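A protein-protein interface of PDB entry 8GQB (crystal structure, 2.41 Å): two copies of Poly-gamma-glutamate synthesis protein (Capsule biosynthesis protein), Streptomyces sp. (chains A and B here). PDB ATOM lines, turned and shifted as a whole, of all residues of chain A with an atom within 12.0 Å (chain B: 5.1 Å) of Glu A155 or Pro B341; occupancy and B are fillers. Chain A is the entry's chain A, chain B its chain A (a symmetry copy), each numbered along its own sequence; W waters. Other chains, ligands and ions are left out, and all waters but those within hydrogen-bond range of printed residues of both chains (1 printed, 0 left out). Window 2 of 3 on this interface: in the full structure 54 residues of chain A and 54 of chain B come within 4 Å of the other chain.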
ATOM      1  N   ALA A 150      27.412   6.224  26.290  1.00  0.00           N
ATOM      2  CA  ALA A 150      26.563   5.076  26.019  1.00  0.00           C
ATOM      3  C   ALA A 150      26.910   4.493  24.659  1.00  0.00           C
ATOM      4  O   ALA A 150      27.282   5.218  23.732  1.00  0.00           O
ATOM      5  CB  ALA A 150      25.074   5.450  26.063  1.00  0.00           C
ATOM      6  N   ASP A 151      26.795   3.176  24.552  1.00  0.00           N
ATOM      7  CA  ASP A 151      27.003   2.490  23.289  1.00  0.00           C
ATOM      8  C   ASP A 151      25.715   2.469  22.478  1.00  0.00           C
ATOM      9  O   ASP A 151      24.617   2.583  23.031  1.00  0.00           O
ATOM     10  CB  ASP A 151      27.493   1.066  23.539  1.00  0.00           C
ATOM     11  CG  ASP A 151      29.007   0.975  23.607  1.00  0.00           C
ATOM     12  OD1 ASP A 151      29.684   1.751  22.899  1.00  0.00           O
ATOM     13  OD2 ASP A 151      29.520   0.127  24.367  1.00  0.00           O
ATOM     14  N   PRO A 152      25.815   2.345  21.157  1.00  0.00           N
ATOM     15  CA  PRO A 152      24.606   2.312  20.328  1.00  0.00           C
ATOM     16  C   PRO A 152      23.810   1.032  20.535  1.00  0.00           C
ATOM     17  O   PRO A 152      24.290   0.039  21.086  1.00  0.00           O
ATOM     18  CB  PRO A 152      25.148   2.394  18.896  1.00  0.00           C
ATOM     19  CG  PRO A 152      26.545   2.922  19.034  1.00  0.00           C
ATOM     20  CD  PRO A 152      27.041   2.400  20.343  1.00  0.00           C
ATOM     21  N   SER A 153      22.563   1.080  20.083  1.00  0.00           N
ATOM     22  CA  SER A 153      21.690  -0.084  20.019  1.00  0.00           C
ATOM     23  C   SER A 153      21.450  -0.381  18.542  1.00  0.00           C
ATOM     24  O   SER A 153      21.930   0.375  17.687  1.00  0.00           O
ATOM     25  CB  SER A 153      20.381   0.178  20.767  1.00  0.00           C
ATOM     26  OG  SER A 153      19.522   1.021  20.020  1.00  0.00           O
ATOM     27  N   PRO A 154      20.749  -1.463  18.188  1.00  0.00           N
ATOM     28  CA  PRO A 154      20.414  -1.662  16.768  1.00  0.00           C
ATOM     29  C   PRO A 154      19.611  -0.520  16.166  1.00  0.00           C
ATOM     30  O   PRO A 154      19.707  -0.283  14.955  1.00  0.00           O
ATOM     31  CB  PRO A 154      19.617  -2.971  16.780  1.00  0.00           C
ATOM     32  CG  PRO A 154      20.157  -3.714  17.945  1.00  0.00           C
ATOM     33  CD  PRO A 154      20.468  -2.672  18.987  1.00  0.00           C
ATOM     34  N   GLU A 155      18.834   0.206  16.973  1.00  0.00           N
ATOM     35  CA  GLU A 155      17.972   1.271  16.472  1.00  0.00           C
ATOM     36  C   GLU A 155      18.478   2.676  16.762  1.00  0.00           C
ATOM     37  O   GLU A 155      18.194   3.589  15.984  1.00  0.00           O
ATOM     38  CB  GLU A 155      16.559   1.142  17.058  1.00  0.00           C
ATOM     39  CG  GLU A 155      15.811  -0.103  16.629  1.00  0.00           C
ATOM     40  CD  GLU A 155      16.159  -1.313  17.467  1.00  0.00           C
ATOM     41  OE1 GLU A 155      16.443  -1.136  18.670  1.00  0.00           O
ATOM     42  OE2 GLU A 155      16.153  -2.437  16.924  1.00  0.00           O
ATOM     43  N   LEU A 156      19.205   2.876  17.859  1.00  0.00           N
ATOM     44  CA  LEU A 156      19.629   4.210  18.248  1.00  0.00           C
ATOM     45  C   LEU A 156      21.148   4.292  18.344  1.00  0.00           C
ATOM     46  O   LEU A 156      21.813   3.301  18.662  1.00  0.00           O
ATOM     47  CB  LEU A 156      19.013   4.617  19.593  1.00  0.00           C
ATOM     48  CG  LEU A 156      17.522   4.955  19.588  1.00  0.00           C
ATOM     49  CD1 LEU A 156      17.066   5.335  20.988  1.00  0.00           C
ATOM     50  CD2 LEU A 156      17.242   6.079  18.602  1.00  0.00           C
ATOM     51  N   PRO A 157      21.725   5.464  18.066  1.00  0.00           N
ATOM     52  CA  PRO A 157      23.167   5.638  18.270  1.00  0.00           C
ATOM     53  C   PRO A 157      23.520   5.704  19.742  1.00  0.00           C
ATOM     54  O   PRO A 157      22.635   5.703  20.603  1.00  0.00           O
ATOM     55  CB  PRO A 157      23.461   6.966  17.563  1.00  0.00           C
ATOM     56  CG  PRO A 157      22.170   7.722  17.660  1.00  0.00           C
ATOM     57  CD  PRO A 157      21.091   6.680  17.524  1.00  0.00           C
ATOM     58  N   GLY A 158      24.811   5.755  20.047  1.00  0.00           N
ATOM     59  CA  GLY A 158      25.263   5.916  21.411  1.00  0.00           C
ATOM     60  C   GLY A 158      25.120   7.351  21.877  1.00  0.00           C
ATOM     61  O   GLY A 158      24.397   8.161  21.290  1.00  0.00           O
ATOM     62  N   ARG A 159      25.828   7.664  22.962  1.00  0.00           N
ATOM     63  CA  ARG A 159      25.824   9.004  23.520  1.00  0.00           C
ATOM     64  C   ARG A 159      27.261   9.374  23.868  1.00  0.00           C
ATOM     65  O   ARG A 159      27.951   8.596  24.554  1.00  0.00           O
ATOM     66  CB  ARG A 159      24.928   9.115  24.759  1.00  0.00           C
ATOM     67  CG  ARG A 159      24.939  10.497  25.401  1.00  0.00           C
ATOM     68  CD  ARG A 159      24.055  10.562  26.637  1.00  0.00           C
ATOM     69  NE  ARG A 159      24.501   9.656  27.693  1.00  0.00           N
ATOM     70  CZ  ARG A 159      23.878   8.529  28.022  1.00  0.00           C
ATOM     71  NH1 ARG A 159      22.773   8.166  27.383  1.00  0.00           N
ATOM     72  NH2 ARG A 159      24.358   7.767  28.998  1.00  0.00           N
ATOM     73  N   THR B 322       7.055   1.943  20.124  1.00  0.00           N
ATOM     74  CA  THR B 322       8.154   2.748  19.612  1.00  0.00           C
ATOM     75  C   THR B 322       9.148   1.871  18.860  1.00  0.00           C
ATOM     76  O   THR B 322       9.419   0.729  19.248  1.00  0.00           O
ATOM     77  CB  THR B 322       8.852   3.507  20.746  1.00  0.00           C
ATOM     78  OG1 THR B 322       9.810   4.419  20.195  1.00  0.00           O
ATOM     79  CG2 THR B 322       9.566   2.558  21.688  1.00  0.00           C
ATOM     80  N   ASP B 323       9.670   2.403  17.759  1.00  0.00           N
ATOM     81  CA  ASP B 323      10.557   1.661  16.876  1.00  0.00           C
ATOM     82  C   ASP B 323      12.029   1.922  17.170  1.00  0.00           C
ATOM     83  O   ASP B 323      12.893   1.454  16.423  1.00  0.00           O
ATOM     84  CB  ASP B 323      10.243   2.004  15.418  1.00  0.00           C
ATOM     85  CG  ASP B 323      10.460   0.831  14.481  1.00  0.00           C
ATOM     86  OD1 ASP B 323      10.764  -0.277  14.971  1.00  0.00           O
ATOM     87  OD2 ASP B 323      10.325   1.019  13.253  1.00  0.00           O
ATOM     88  N   ARG B 324      12.334   2.653  18.243  1.00  0.00           N
ATOM     89  CA  ARG B 324      13.711   3.018  18.576  1.00  0.00           C
ATOM     90  C   ARG B 324      13.895   2.866  20.084  1.00  0.00           C
ATOM     91  O   ARG B 324      13.456   3.720  20.859  1.00  0.00           O
ATOM     92  CB  ARG B 324      14.028   4.436  18.118  1.00  0.00           C
ATOM     93  N   VAL B 325      14.549   1.781  20.490  1.00  0.00           N
ATOM     94  CA  VAL B 325      14.861   1.510  21.890  1.00  0.00           C
ATOM     95  C   VAL B 325      16.367   1.640  22.073  1.00  0.00           C
ATOM     96  O   VAL B 325      17.144   1.052  21.311  1.00  0.00           O
ATOM     97  CB  VAL B 325      14.365   0.117  22.316  1.00  0.00           C
ATOM     98  CG1 VAL B 325      14.753  -0.173  23.758  1.00  0.00           C
ATOM     99  CG2 VAL B 325      12.858   0.012  22.131  1.00  0.00           C
ATOM    100  N   TYR B 330      17.452  -1.408  26.533  1.00  0.00           N
ATOM    101  CA  TYR B 330      17.571  -2.846  26.300  1.00  0.00           C
ATOM    102  C   TYR B 330      18.260  -3.547  27.463  1.00  0.00           C
ATOM    103  O   TYR B 330      17.927  -4.694  27.780  1.00  0.00           O
ATOM    104  CB  TYR B 330      18.336  -3.119  25.004  1.00  0.00           C
ATOM    105  CG  TYR B 330      17.499  -3.057  23.746  1.00  0.00           C
ATOM    106  CD1 TYR B 330      16.429  -3.923  23.556  1.00  0.00           C
ATOM    107  CD2 TYR B 330      17.799  -2.153  22.734  1.00  0.00           C
ATOM    108  CE1 TYR B 330      15.668  -3.878  22.403  1.00  0.00           C
ATOM    109  CE2 TYR B 330      17.045  -2.102  21.577  1.00  0.00           C
ATOM    110  CZ  TYR B 330      15.980  -2.965  21.416  1.00  0.00           C
ATOM    111  OH  TYR B 330      15.229  -2.915  20.267  1.00  0.00           O
ATOM    112  N   LEU B 339      17.518  -8.484  21.228  1.00  0.00           N
ATOM    113  CA  LEU B 339      16.076  -8.311  21.287  1.00  0.00           C
ATOM    114  C   LEU B 339      15.617  -7.245  20.302  1.00  0.00           C
ATOM    115  O   LEU B 339      16.268  -6.209  20.139  1.00  0.00           O
ATOM    116  CB  LEU B 339      15.630  -7.928  22.702  1.00  0.00           C
ATOM    117  CG  LEU B 339      14.864  -8.995  23.484  1.00  0.00           C
ATOM    118  CD1 LEU B 339      15.600 -10.324  23.439  1.00  0.00           C
ATOM    119  CD2 LEU B 339      14.647  -8.548  24.921  1.00  0.00           C
ATOM    120  N   THR B 340      14.494  -7.515  19.647  1.00  0.00           N
ATOM    121  CA  THR B 340      13.804  -6.518  18.851  1.00  0.00           C
ATOM    122  C   THR B 340      12.935  -5.654  19.764  1.00  0.00           C
ATOM    123  O   THR B 340      12.613  -6.059  20.884  1.00  0.00           O
ATOM    124  CB  THR B 340      12.959  -7.204  17.779  1.00  0.00           C
ATOM    125  OG1 THR B 340      12.028  -8.100  18.398  1.00  0.00           O
ATOM    126  CG2 THR B 340      13.851  -7.991  16.824  1.00  0.00           C
ATOM    127  N   PRO B 341      12.562  -4.446  19.321  1.00  0.00           N
ATOM    128  CA  PRO B 341      11.801  -3.551  20.220  1.00  0.00           C
ATOM    129  C   PRO B 341      10.524  -4.169  20.772  1.00  0.00           C
ATOM    130  O   PRO B 341      10.257  -4.060  21.977  1.00  0.00           O
ATOM    131  CB  PRO B 341      11.515  -2.334  19.329  1.00  0.00           C
ATOM    132  CG  PRO B 341      12.620  -2.330  18.338  1.00  0.00           C
ATOM    133  CD  PRO B 341      12.926  -3.774  18.060  1.00  0.00           C
ATOM    134  N   GLY B 342       9.726  -4.816  19.920  1.00  0.00           N
ATOM    135  CA  GLY B 342       8.477  -5.398  20.388  1.00  0.00           C
ATOM    136  C   GLY B 342       8.689  -6.509  21.399  1.00  0.00           C
ATOM    137  O   GLY B 342       7.994  -6.576  22.416  1.00  0.00           O
ATOM    138  N   ARG B 343       9.651  -7.397  21.135  1.00  0.00           N
ATOM    139  CA  ARG B 343       9.975  -8.440  22.105  1.00  0.00           C
ATOM    140  C   ARG B 343      10.517  -7.843  23.398  1.00  0.00           C
ATOM    141  O   ARG B 343      10.236  -8.350  24.492  1.00  0.00           O
ATOM    142  CB  ARG B 343      10.983  -9.424  21.513  1.00  0.00           C
ATOM    143  CG  ARG B 343      10.444 -10.281  20.380  1.00  0.00           C
ATOM    144  CD  ARG B 343      11.483 -11.302  19.939  1.00  0.00           C
ATOM    145  NE  ARG B 343      10.961 -12.247  18.955  1.00  0.00           N
ATOM    146  CZ  ARG B 343      11.080 -12.099  17.640  1.00  0.00           C
ATOM    147  NH1 ARG B 343      11.703 -11.039  17.144  1.00  0.00           N
ATOM    148  NH2 ARG B 343      10.576 -13.013  16.820  1.00  0.00           N
ATOM    149  N   TYR B 344      11.303  -6.767  23.292  1.00  0.00           N
ATOM    150  CA  TYR B 344      11.803  -6.092  24.485  1.00  0.00           C
ATOM    151  C   TYR B 344      10.657  -5.566  25.339  1.00  0.00           C
ATOM    152  O   TYR B 344      10.653  -5.736  26.562  1.00  0.00           O
ATOM    153  CB  TYR B 344      12.745  -4.953  24.094  1.00  0.00           C
ATOM    154  CG  TYR B 344      12.838  -3.868  25.144  1.00  0.00           C
ATOM    155  CD1 TYR B 344      13.601  -4.049  26.290  1.00  0.00           C
ATOM    156  CD2 TYR B 344      12.158  -2.664  24.990  1.00  0.00           C
ATOM    157  CE1 TYR B 344      13.684  -3.063  27.255  1.00  0.00           C
ATOM    158  CE2 TYR B 344      12.236  -1.672  25.950  1.00  0.00           C
ATOM    159  CZ  TYR B 344      13.003  -1.875  27.081  1.00  0.00           C
ATOM    160  OH  TYR B 344      13.084  -0.890  28.039  1.00  0.00           O
ATOM    161  N   TYR B 345       9.672  -4.916  24.711  1.00  0.00           N
ATOM    162  CA  TYR B 345       8.543  -4.397  25.478  1.00  0.00           C
ATOM    163  C   TYR B 345       7.647  -5.515  25.990  1.00  0.00           C
ATOM    164  O   TYR B 345       7.006  -5.363  27.037  1.00  0.00           O
ATOM    165  CB  TYR B 345       7.736  -3.408  24.640  1.00  0.00           C
ATOM    166  CG  TYR B 345       8.316  -2.015  24.667  1.00  0.00           C
ATOM    167  CD1 TYR B 345       8.122  -1.187  25.764  1.00  0.00           C
ATOM    168  CD2 TYR B 345       9.070  -1.536  23.606  1.00  0.00           C
ATOM    169  CE1 TYR B 345       8.655   0.085  25.800  1.00  0.00           C
ATOM    170  CE2 TYR B 345       9.608  -0.267  23.633  1.00  0.00           C
ATOM    171  CZ  TYR B 345       9.397   0.540  24.732  1.00  0.00           C
ATOM    172  OH  TYR B 345       9.930   1.806  24.762  1.00  0.00           O
ATOM    173  N   ASP B 346       7.585  -6.638  25.273  1.00  0.00           N
ATOM    174  CA  ASP B 346       6.817  -7.775  25.760  1.00  0.00           C
ATOM    175  C   ASP B 346       7.445  -8.352  27.022  1.00  0.00           C
ATOM    176  O   ASP B 346       6.754  -8.602  28.015  1.00  0.00           O
ATOM    177  CB  ASP B 346       6.709  -8.842  24.669  1.00  0.00           C
ATOM    178  CG  ASP B 346       5.698  -9.918  25.007  1.00  0.00           C
ATOM    179  OD1 ASP B 346       4.493  -9.598  25.076  1.00  0.00           O
ATOM    180  OD2 ASP B 346       6.107 -11.083  25.199  1.00  0.00           O
HETATM  181  O   HOH W   1      17.021  -4.964  17.585  1.00  0.00           O
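OG of Ser A153 is in hydrogen-bond range of O of Val B325, at 2.7 Å.
The side-chain hydroxyl (OH) of Tyr B330 sits at hydrogen-bond distance from the side-chain carboxylate (OE1) of Glu A155 (2.7 Å).
Of the 13 printed residues of chain B, 5 touch a printed residue of chain A.
Hydrophobic or aromatic side chains of chain B within 4 Å of the printed part of chain A: Tyr B330 and Pro B341.
Of the 10 printed residues of chain A, 3 touch a printed residue of chain B.
Hydrophobic or aromatic side chains of chain A that line the printed part of chain B: Leu A156.
Along chain A the printed residues that touch a printed residue of chain B span positions 153 to 156.
Among the printed residues, 9 pairs touch across the chains.
Among the printed residues, no Asp or Glu carboxylate lies within 4 Å of a Lys or Arg side-chain nitrogen of the other chain.
Water W1 lies within hydrogen-bond range of OE2 of Glu A155 (2.8 Å) and O of Leu B339 (2.9 Å).
No position is printed for both chains.
Tyr B330 touches Ser A153 (CD2 to CB, 3.996 Å).
Asp B323 touches Glu A155 (O to CG, 3.3 Å).
Glu A155 touches Arg B324 (CB to CA, 3.7 Å).
OE1 of Glu A155 touches O of Val B325, 3.5 Å away.
Pro B341 touches Glu A155.
Arg B324 touches Leu A156.
C of Val B325 touches CD1 of Leu A156, 3.9 Å away.
N of Glu A155 sits close to OG of Ser A153 (3.2 Å).
OG of Ser A153 is in hydrogen-bond range of N of Leu A156 (2.9 Å).
The side-chain hydroxyl (OH) of Tyr B330 lies close to the backbone carbonyl oxygen (O) of Leu B339 (3.5 Å).
Of the printed residues of chain B, Ser A153 touches Val B325 and Tyr B330.
Glu A155 touches just these residues of chain B: Asp B323 (3.3 Å), Arg B324 (3.7 Å), Val B325 (3.5 Å), Tyr B330 (2.7 Å) and Pro B341 (3.7 Å).
Of the printed residues of chain B, Leu A156 touches Arg B324 (3.6 Å) and Val B325 (3.9 Å).
No residue of chain A comes within 4 Å of Thr B322.
Asp B323 touches one residue of chain A.
Arg B324 touches just these residues of chain A: Glu A155 and Leu A156.
Printed residues of chain A within 4 Å of Tyr B330: Ser A153 (3.996 Å) and Glu A155 (2.7 Å).
Thr B340 touches none of the printed residues of chain A.
Printed residues of chain A within 4 Å of Pro B341: Glu A155 (3.7 Å).
No residue of chain A comes within 4 Å of Gly B342.
Tyr B344 touches none of the printed residues of chain A.
The nearest residue of chain B that does not touch Glu A155 is Leu B339 (5.0 Å).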
